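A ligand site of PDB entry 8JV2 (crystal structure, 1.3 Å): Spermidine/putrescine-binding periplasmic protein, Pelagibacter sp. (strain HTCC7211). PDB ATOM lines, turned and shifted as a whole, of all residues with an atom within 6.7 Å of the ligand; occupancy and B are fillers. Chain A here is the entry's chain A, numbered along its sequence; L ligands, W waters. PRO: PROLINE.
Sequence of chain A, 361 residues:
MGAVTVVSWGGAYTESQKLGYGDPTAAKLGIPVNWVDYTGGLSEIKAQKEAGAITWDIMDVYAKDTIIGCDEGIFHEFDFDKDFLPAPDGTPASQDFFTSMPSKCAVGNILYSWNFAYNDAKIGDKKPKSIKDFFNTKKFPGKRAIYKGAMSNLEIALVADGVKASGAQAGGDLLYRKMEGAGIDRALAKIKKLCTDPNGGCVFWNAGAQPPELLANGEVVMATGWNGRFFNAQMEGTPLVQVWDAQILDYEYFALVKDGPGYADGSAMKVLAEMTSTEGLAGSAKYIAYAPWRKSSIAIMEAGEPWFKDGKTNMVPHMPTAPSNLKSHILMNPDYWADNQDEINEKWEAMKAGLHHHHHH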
ATOM      1  N   SER A   8     -14.815 -33.267   1.476  1.00  0.00           N
ATOM      2  CA  SER A   8     -14.006 -32.161   1.969  1.00  0.00           C
ATOM      3  C   SER A   8     -14.294 -30.912   1.126  1.00  0.00           C
ATOM      4  O   SER A   8     -15.288 -30.850   0.415  1.00  0.00           O
ATOM      5  CB  SER A   8     -12.535 -32.555   2.049  1.00  0.00           C
ATOM      6  OG  SER A   8     -11.847 -31.579   2.823  1.00  0.00           O
ATOM      7  N   TRP A   9     -13.439 -29.904   1.259  1.00  0.00           N
ATOM      8  CA  TRP A   9     -13.810 -28.523   0.949  1.00  0.00           C
ATOM      9  C   TRP A   9     -13.280 -28.047  -0.389  1.00  0.00           C
ATOM     10  O   TRP A   9     -13.533 -26.902  -0.781  1.00  0.00           O
ATOM     11  CB  TRP A   9     -13.365 -27.595   2.073  1.00  0.00           C
ATOM     12  CG  TRP A   9     -13.924 -27.978   3.425  1.00  0.00           C
ATOM     13  CD1 TRP A   9     -13.631 -29.114   4.142  1.00  0.00           C
ATOM     14  CD2 TRP A   9     -14.872 -27.259   4.234  1.00  0.00           C
ATOM     15  NE1 TRP A   9     -14.339 -29.145   5.318  1.00  0.00           N
ATOM     16  CE2 TRP A   9     -15.093 -28.007   5.413  1.00  0.00           C
ATOM     17  CE3 TRP A   9     -15.528 -26.038   4.095  1.00  0.00           C
ATOM     18  CZ2 TRP A   9     -15.963 -27.605   6.417  1.00  0.00           C
ATOM     19  CZ3 TRP A   9     -16.389 -25.618   5.107  1.00  0.00           C
ATOM     20  CH2 TRP A   9     -16.582 -26.403   6.257  1.00  0.00           C
ATOM     21  N   GLY A  10     -12.583 -28.918  -1.124  1.00  0.00           N
ATOM     22  CA  GLY A  10     -12.145 -28.601  -2.460  1.00  0.00           C
ATOM     23  C   GLY A  10     -10.848 -27.823  -2.521  1.00  0.00           C
ATOM     24  O   GLY A  10     -10.168 -27.553  -1.521  1.00  0.00           O
ATOM     25  N   ALA A  12      -7.326 -26.174  -2.781  1.00  0.00           N
ATOM     26  CA  ALA A  12      -6.026 -26.466  -2.189  1.00  0.00           C
ATOM     27  C   ALA A  12      -6.148 -27.352  -0.965  1.00  0.00           C
ATOM     28  O   ALA A  12      -5.224 -28.102  -0.649  1.00  0.00           O
ATOM     29  CB  ALA A  12      -5.315 -25.170  -1.816  1.00  0.00           C
ATOM     30  N   TYR A  13      -7.276 -27.273  -0.239  1.00  0.00           N
ATOM     31  CA  TYR A  13      -7.413 -28.081   0.952  1.00  0.00           C
ATOM     32  C   TYR A  13      -7.571 -29.553   0.591  1.00  0.00           C
ATOM     33  O   TYR A  13      -6.800 -30.407   1.059  1.00  0.00           O
ATOM     34  CB  TYR A  13      -8.538 -27.564   1.850  1.00  0.00           C
ATOM     35  CG  TYR A  13      -8.639 -28.362   3.131  1.00  0.00           C
ATOM     36  CD1 TYR A  13      -7.530 -28.536   3.945  1.00  0.00           C
ATOM     37  CD2 TYR A  13      -9.849 -28.920   3.539  1.00  0.00           C
ATOM     38  CE1 TYR A  13      -7.600 -29.269   5.100  1.00  0.00           C
ATOM     39  CE2 TYR A  13      -9.934 -29.653   4.710  1.00  0.00           C
ATOM     40  CZ  TYR A  13      -8.802 -29.835   5.492  1.00  0.00           C
ATOM     41  OH  TYR A  13      -8.823 -30.558   6.655  1.00  0.00           O
ATOM     42  N   THR A  14      -8.542 -29.899  -0.257  1.00  0.00           N
ATOM     43  CA  THR A  14      -8.659 -31.289  -0.673  1.00  0.00           C
ATOM     44  C   THR A  14      -7.358 -31.783  -1.290  1.00  0.00           C
ATOM     45  O   THR A  14      -6.959 -32.925  -1.068  1.00  0.00           O
ATOM     46  CB  THR A  14      -9.839 -31.466  -1.628  1.00  0.00           C
ATOM     47  OG1 THR A  14     -11.054 -31.298  -0.882  1.00  0.00           O
ATOM     48  CG2 THR A  14      -9.819 -32.860  -2.277  1.00  0.00           C
ATOM     49  N   ASP A  60     -15.006 -34.377   6.348  1.00  0.00           N
ATOM     50  CA  ASP A  60     -14.176 -33.353   6.966  1.00  0.00           C
ATOM     51  C   ASP A  60     -15.108 -32.217   7.348  1.00  0.00           C
ATOM     52  O   ASP A  60     -15.744 -31.619   6.472  1.00  0.00           O
ATOM     53  CB  ASP A  60     -13.133 -32.911   5.944  1.00  0.00           C
ATOM     54  CG  ASP A  60     -12.172 -31.897   6.501  1.00  0.00           C
ATOM     55  OD1 ASP A  60     -12.668 -30.796   6.839  1.00  0.00           O
ATOM     56  OD2 ASP A  60     -10.949 -32.181   6.567  1.00  0.00           O
ATOM     57  N   VAL A  61     -15.237 -31.954   8.644  1.00  0.00           N
ATOM     58  CA  VAL A  61     -16.311 -31.128   9.186  1.00  0.00           C
ATOM     59  C   VAL A  61     -15.806 -30.057  10.137  1.00  0.00           C
ATOM     60  O   VAL A  61     -14.830 -30.222  10.877  1.00  0.00           O
ATOM     61  CB  VAL A  61     -17.389 -31.969   9.901  1.00  0.00           C
ATOM     62  CG1 VAL A  61     -18.119 -32.832   8.913  1.00  0.00           C
ATOM     63  CG2 VAL A  61     -16.796 -32.805  11.017  1.00  0.00           C
ATOM     64  N   TYR A  62     -16.552 -28.953  10.142  1.00  0.00           N
ATOM     65  CA  TYR A  62     -16.458 -27.960  11.181  1.00  0.00           C
ATOM     66  C   TYR A  62     -16.553 -28.602  12.562  1.00  0.00           C
ATOM     67  O   TYR A  62     -17.312 -29.556  12.787  1.00  0.00           O
ATOM     68  CB  TYR A  62     -17.637 -26.998  11.083  1.00  0.00           C
ATOM     69  CG  TYR A  62     -17.614 -25.903  10.050  1.00  0.00           C
ATOM     70  CD1 TYR A  62     -16.493 -25.105   9.884  1.00  0.00           C
ATOM     71  CD2 TYR A  62     -18.751 -25.597   9.316  1.00  0.00           C
ATOM     72  CE1 TYR A  62     -16.488 -24.046   9.007  1.00  0.00           C
ATOM     73  CE2 TYR A  62     -18.764 -24.522   8.421  1.00  0.00           C
ATOM     74  CZ  TYR A  62     -17.608 -23.755   8.277  1.00  0.00           C
ATOM     75  OH  TYR A  62     -17.570 -22.684   7.411  1.00  0.00           O
ATOM     76  N   ASN A 109      -7.854 -33.585  12.334  1.00  0.00           N
ATOM     77  CA  ASN A 109      -6.857 -33.634  11.278  1.00  0.00           C
ATOM     78  C   ASN A 109      -5.897 -32.452  11.371  1.00  0.00           C
ATOM     79  O   ASN A 109      -4.744 -32.657  11.769  1.00  0.00           O
ATOM     80  CB  ASN A 109      -7.433 -33.879   9.866  1.00  0.00           C
ATOM     81  CG  ASN A 109      -8.627 -33.001   9.504  1.00  0.00           C
ATOM     82  OD1 ASN A 109      -8.793 -31.894   9.979  1.00  0.00           O
ATOM     83  ND2 ASN A 109      -9.446 -33.506   8.593  1.00  0.00           N
ATOM     84  N   ILE A 110      -6.360 -31.229  11.100  1.00  0.00           N
ATOM     85  CA  ILE A 110      -5.497 -30.057  11.134  1.00  0.00           C
ATOM     86  C   ILE A 110      -6.157 -28.912  11.905  1.00  0.00           C
ATOM     87  O   ILE A 110      -7.359 -28.934  12.208  1.00  0.00           O
ATOM     88  CB  ILE A 110      -5.020 -29.602   9.728  1.00  0.00           C
ATOM     89  CG1 ILE A 110      -6.185 -29.315   8.767  1.00  0.00           C
ATOM     90  CG2 ILE A 110      -4.132 -30.678   9.121  1.00  0.00           C
ATOM     91  CD1 ILE A 110      -6.968 -28.017   9.003  1.00  0.00           C
ATOM     92  N   TYR A 112      -6.549 -24.645  11.561  1.00  0.00           N
ATOM     93  CA  TYR A 112      -6.592 -23.625  10.528  1.00  0.00           C
ATOM     94  C   TYR A 112      -7.023 -22.311  11.143  1.00  0.00           C
ATOM     95  O   TYR A 112      -7.584 -22.285  12.235  1.00  0.00           O
ATOM     96  CB  TYR A 112      -7.568 -23.996   9.406  1.00  0.00           C
ATOM     97  CG  TYR A 112      -9.031 -24.121   9.754  1.00  0.00           C
ATOM     98  CD1 TYR A 112      -9.521 -25.157  10.545  1.00  0.00           C
ATOM     99  CD2 TYR A 112      -9.946 -23.223   9.237  1.00  0.00           C
ATOM    100  CE1 TYR A 112     -10.888 -25.287  10.787  1.00  0.00           C
ATOM    101  CE2 TYR A 112     -11.291 -23.346   9.462  1.00  0.00           C
ATOM    102  CZ  TYR A 112     -11.763 -24.371  10.245  1.00  0.00           C
ATOM    103  OH  TYR A 112     -13.124 -24.508  10.456  1.00  0.00           O
ATOM    104  N   GLY A 208     -14.122 -22.025  -0.180  1.00  0.00           N
ATOM    105  CA  GLY A 208     -12.836 -21.574   0.330  1.00  0.00           C
ATOM    106  C   GLY A 208     -11.962 -20.891  -0.689  1.00  0.00           C
ATOM    107  O   GLY A 208     -11.106 -20.080  -0.325  1.00  0.00           O
ATOM    108  N   TRP A 226      -9.776 -18.478   4.820  1.00  0.00           N
ATOM    109  CA  TRP A 226      -8.983 -19.439   5.562  1.00  0.00           C
ATOM    110  C   TRP A 226      -7.521 -19.328   5.134  1.00  0.00           C
ATOM    111  O   TRP A 226      -7.213 -19.228   3.944  1.00  0.00           O
ATOM    112  CB  TRP A 226      -9.538 -20.856   5.342  1.00  0.00           C
ATOM    113  CG  TRP A 226     -10.941 -20.992   5.839  1.00  0.00           C
ATOM    114  CD1 TRP A 226     -11.435 -20.558   7.041  1.00  0.00           C
ATOM    115  CD2 TRP A 226     -12.037 -21.610   5.166  1.00  0.00           C
ATOM    116  NE1 TRP A 226     -12.768 -20.867   7.153  1.00  0.00           N
ATOM    117  CE2 TRP A 226     -13.165 -21.517   6.008  1.00  0.00           C
ATOM    118  CE3 TRP A 226     -12.189 -22.251   3.926  1.00  0.00           C
ATOM    119  CZ2 TRP A 226     -14.410 -22.015   5.653  1.00  0.00           C
ATOM    120  CZ3 TRP A 226     -13.439 -22.744   3.579  1.00  0.00           C
ATOM    121  CH2 TRP A 226     -14.532 -22.615   4.434  1.00  0.00           C
ATOM    122  N   ASN A 227      -6.625 -19.327   6.108  1.00  0.00           N
ATOM    123  CA  ASN A 227      -5.242 -18.932   5.834  1.00  0.00           C
ATOM    124  C   ASN A 227      -4.594 -19.830   4.802  1.00  0.00           C
ATOM    125  O   ASN A 227      -3.737 -19.367   4.028  1.00  0.00           O
ATOM    126  CB  ASN A 227      -4.401 -18.892   7.105  1.00  0.00           C
ATOM    127  CG  ASN A 227      -4.024 -20.277   7.593  1.00  0.00           C
ATOM    128  OD1 ASN A 227      -4.820 -20.968   8.214  1.00  0.00           O
ATOM    129  ND2 ASN A 227      -2.792 -20.680   7.302  1.00  0.00           N
ATOM    130  N   GLY A 228      -4.965 -21.113   4.765  1.00  0.00           N
ATOM    131  CA  GLY A 228      -4.353 -22.032   3.822  1.00  0.00           C
ATOM    132  C   GLY A 228      -4.715 -21.734   2.387  1.00  0.00           C
ATOM    133  O   GLY A 228      -3.938 -22.014   1.472  1.00  0.00           O
ATOM    134  N   ARG A 229      -5.910 -21.186   2.172  1.00  0.00           N
ATOM    135  CA  ARG A 229      -6.319 -20.793   0.838  1.00  0.00           C
ATOM    136  C   ARG A 229      -5.533 -19.573   0.363  1.00  0.00           C
ATOM    137  O   ARG A 229      -5.139 -19.508  -0.813  1.00  0.00           O
ATOM    138  CB  ARG A 229      -7.831 -20.535   0.814  1.00  0.00           C
ATOM    139  CG  ARG A 229      -8.661 -21.743   1.259  1.00  0.00           C
ATOM    140  CD  ARG A 229      -8.364 -22.995   0.431  1.00  0.00           C
ATOM    141  NE  ARG A 229      -9.411 -23.962   0.742  1.00  0.00           N
ATOM    142  CZ  ARG A 229     -10.342 -24.408  -0.085  1.00  0.00           C
ATOM    143  NH1 ARG A 229     -10.345 -24.104  -1.380  1.00  0.00           N
ATOM    144  NH2 ARG A 229     -11.307 -25.165   0.416  1.00  0.00           N
ATOM    145  N   GLU A 252     -10.073 -28.547  12.931  1.00  0.00           N
ATOM    146  CA  GLU A 252     -10.850 -29.328  11.965  1.00  0.00           C
ATOM    147  C   GLU A 252     -10.779 -30.806  12.297  1.00  0.00           C
ATOM    148  O   GLU A 252      -9.830 -31.282  12.938  1.00  0.00           O
ATOM    149  CB  GLU A 252     -10.371 -29.048  10.535  1.00  0.00           C
ATOM    150  CG  GLU A 252     -11.336 -29.481   9.448  1.00  0.00           C
ATOM    151  CD  GLU A 252     -12.609 -28.637   9.344  1.00  0.00           C
ATOM    152  OE1 GLU A 252     -12.827 -27.718  10.165  1.00  0.00           O
ATOM    153  OE2 GLU A 252     -13.426 -28.905   8.405  1.00  0.00           O
ATOM    154  N   ILE A 288       0.131 -27.400   2.393  1.00  0.00           N
ATOM    155  CA  ILE A 288      -0.681 -26.261   2.789  1.00  0.00           C
ATOM    156  C   ILE A 288      -0.325 -25.902   4.226  1.00  0.00           C
ATOM    157  O   ILE A 288       0.099 -26.753   5.012  1.00  0.00           O
ATOM    158  CB  ILE A 288      -2.189 -26.593   2.621  1.00  0.00           C
ATOM    159  CG1 ILE A 288      -3.057 -25.330   2.606  1.00  0.00           C
ATOM    160  CG2 ILE A 288      -2.654 -27.593   3.692  1.00  0.00           C
ATOM    161  CD1 ILE A 288      -4.443 -25.575   2.029  1.00  0.00           C
ATOM    162  N   TYR A 290      -1.562 -25.607   7.143  1.00  0.00           N
ATOM    163  CA  TYR A 290      -2.457 -26.032   8.212  1.00  0.00           C
ATOM    164  C   TYR A 290      -1.680 -26.977   9.122  1.00  0.00           C
ATOM    165  O   TYR A 290      -0.922 -27.832   8.646  1.00  0.00           O
ATOM    166  CB  TYR A 290      -3.700 -26.719   7.666  1.00  0.00           C
ATOM    167  CG  TYR A 290      -4.656 -25.802   6.920  1.00  0.00           C
ATOM    168  CD1 TYR A 290      -4.826 -24.467   7.296  1.00  0.00           C
ATOM    169  CD2 TYR A 290      -5.423 -26.275   5.861  1.00  0.00           C
ATOM    170  CE1 TYR A 290      -5.726 -23.637   6.634  1.00  0.00           C
ATOM    171  CE2 TYR A 290      -6.325 -25.456   5.191  1.00  0.00           C
ATOM    172  CZ  TYR A 290      -6.463 -24.135   5.590  1.00  0.00           C
ATOM    173  OH  TYR A 290      -7.330 -23.294   4.954  1.00  0.00           O
HETATM  174  N   PRO L   1     -11.970 -25.579   5.660  1.00  0.00           N
HETATM  175  CA  PRO L   1     -10.651 -24.968   5.408  1.00  0.00           C
HETATM  176  C   PRO L   1     -10.325 -24.994   3.931  1.00  0.00           C
HETATM  177  O   PRO L   1     -11.158 -25.511   3.178  1.00  0.00           O
HETATM  178  CB  PRO L   1      -9.685 -25.868   6.212  1.00  0.00           C
HETATM  179  CG  PRO L   1     -10.551 -26.693   7.095  1.00  0.00           C
HETATM  180  CD  PRO L   1     -11.789 -26.897   6.295  1.00  0.00           C
HETATM  181  OXT PRO L   1      -9.265 -24.491   3.530  1.00  0.00           O
HETATM  182  O   HOH W   1     -13.773 -24.882   7.587  1.00  0.00           O
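NH2 of Arg 229 lies within salt-bridge range of O of the ligand (2.8 Å).
OH of Tyr 290 sits at hydrogen-bond distance from OXT of the ligand (2.7 Å).
O of Glu 252 lies within hydrogen-bond range of N of Asn 109, at 3.1 Å.
OE2 of Glu 252 lies close to OD1 of Asp 60, 2.6 Å away.
The side-chain carboxylate (OE2) of Glu 252 sits at hydrogen-bond distance from the indole nitrogen (NE1) of Trp 9, at 3.2 Å.
OH of Tyr 290 sits at hydrogen-bond distance from N of Gly 228 (3.2 Å).
The side-chain hydroxyl of Thr 14 is in hydrogen-bond range of the backbone NH of Trp 9, 3.5 Å away.
OH of Tyr 112 sits close to OE1 of Glu 252.
The side-chain hydroxyl (OH) of Tyr 13 is in hydrogen-bond range of the side-chain carboxylate (OD2) of Asp 60, 2.7 Å away.
The guanidinium group (NH2) of Arg 229 sits at hydrogen-bond distance from the backbone carbonyl oxygen (O) of Gly 10 (3.3 Å).
Merely in contact with the ligand: Trp 9, Tyr 13, Tyr 112, Trp 226 and Glu 252.
Hydrophobic or aromatic side chains that line the ligand: Trp 9, Tyr 13, Tyr 112, Trp 226 and Tyr 290.
Along chain A the residues within 4 Å of the ligand span positions 9 to 290.
The nearest printed residue that does not touch the ligand is Asp 60 (4.03 Å).
Water W1 bridges a nitrogen (N) of the ligand and the side-chain hydroxyl of Tyr 112.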
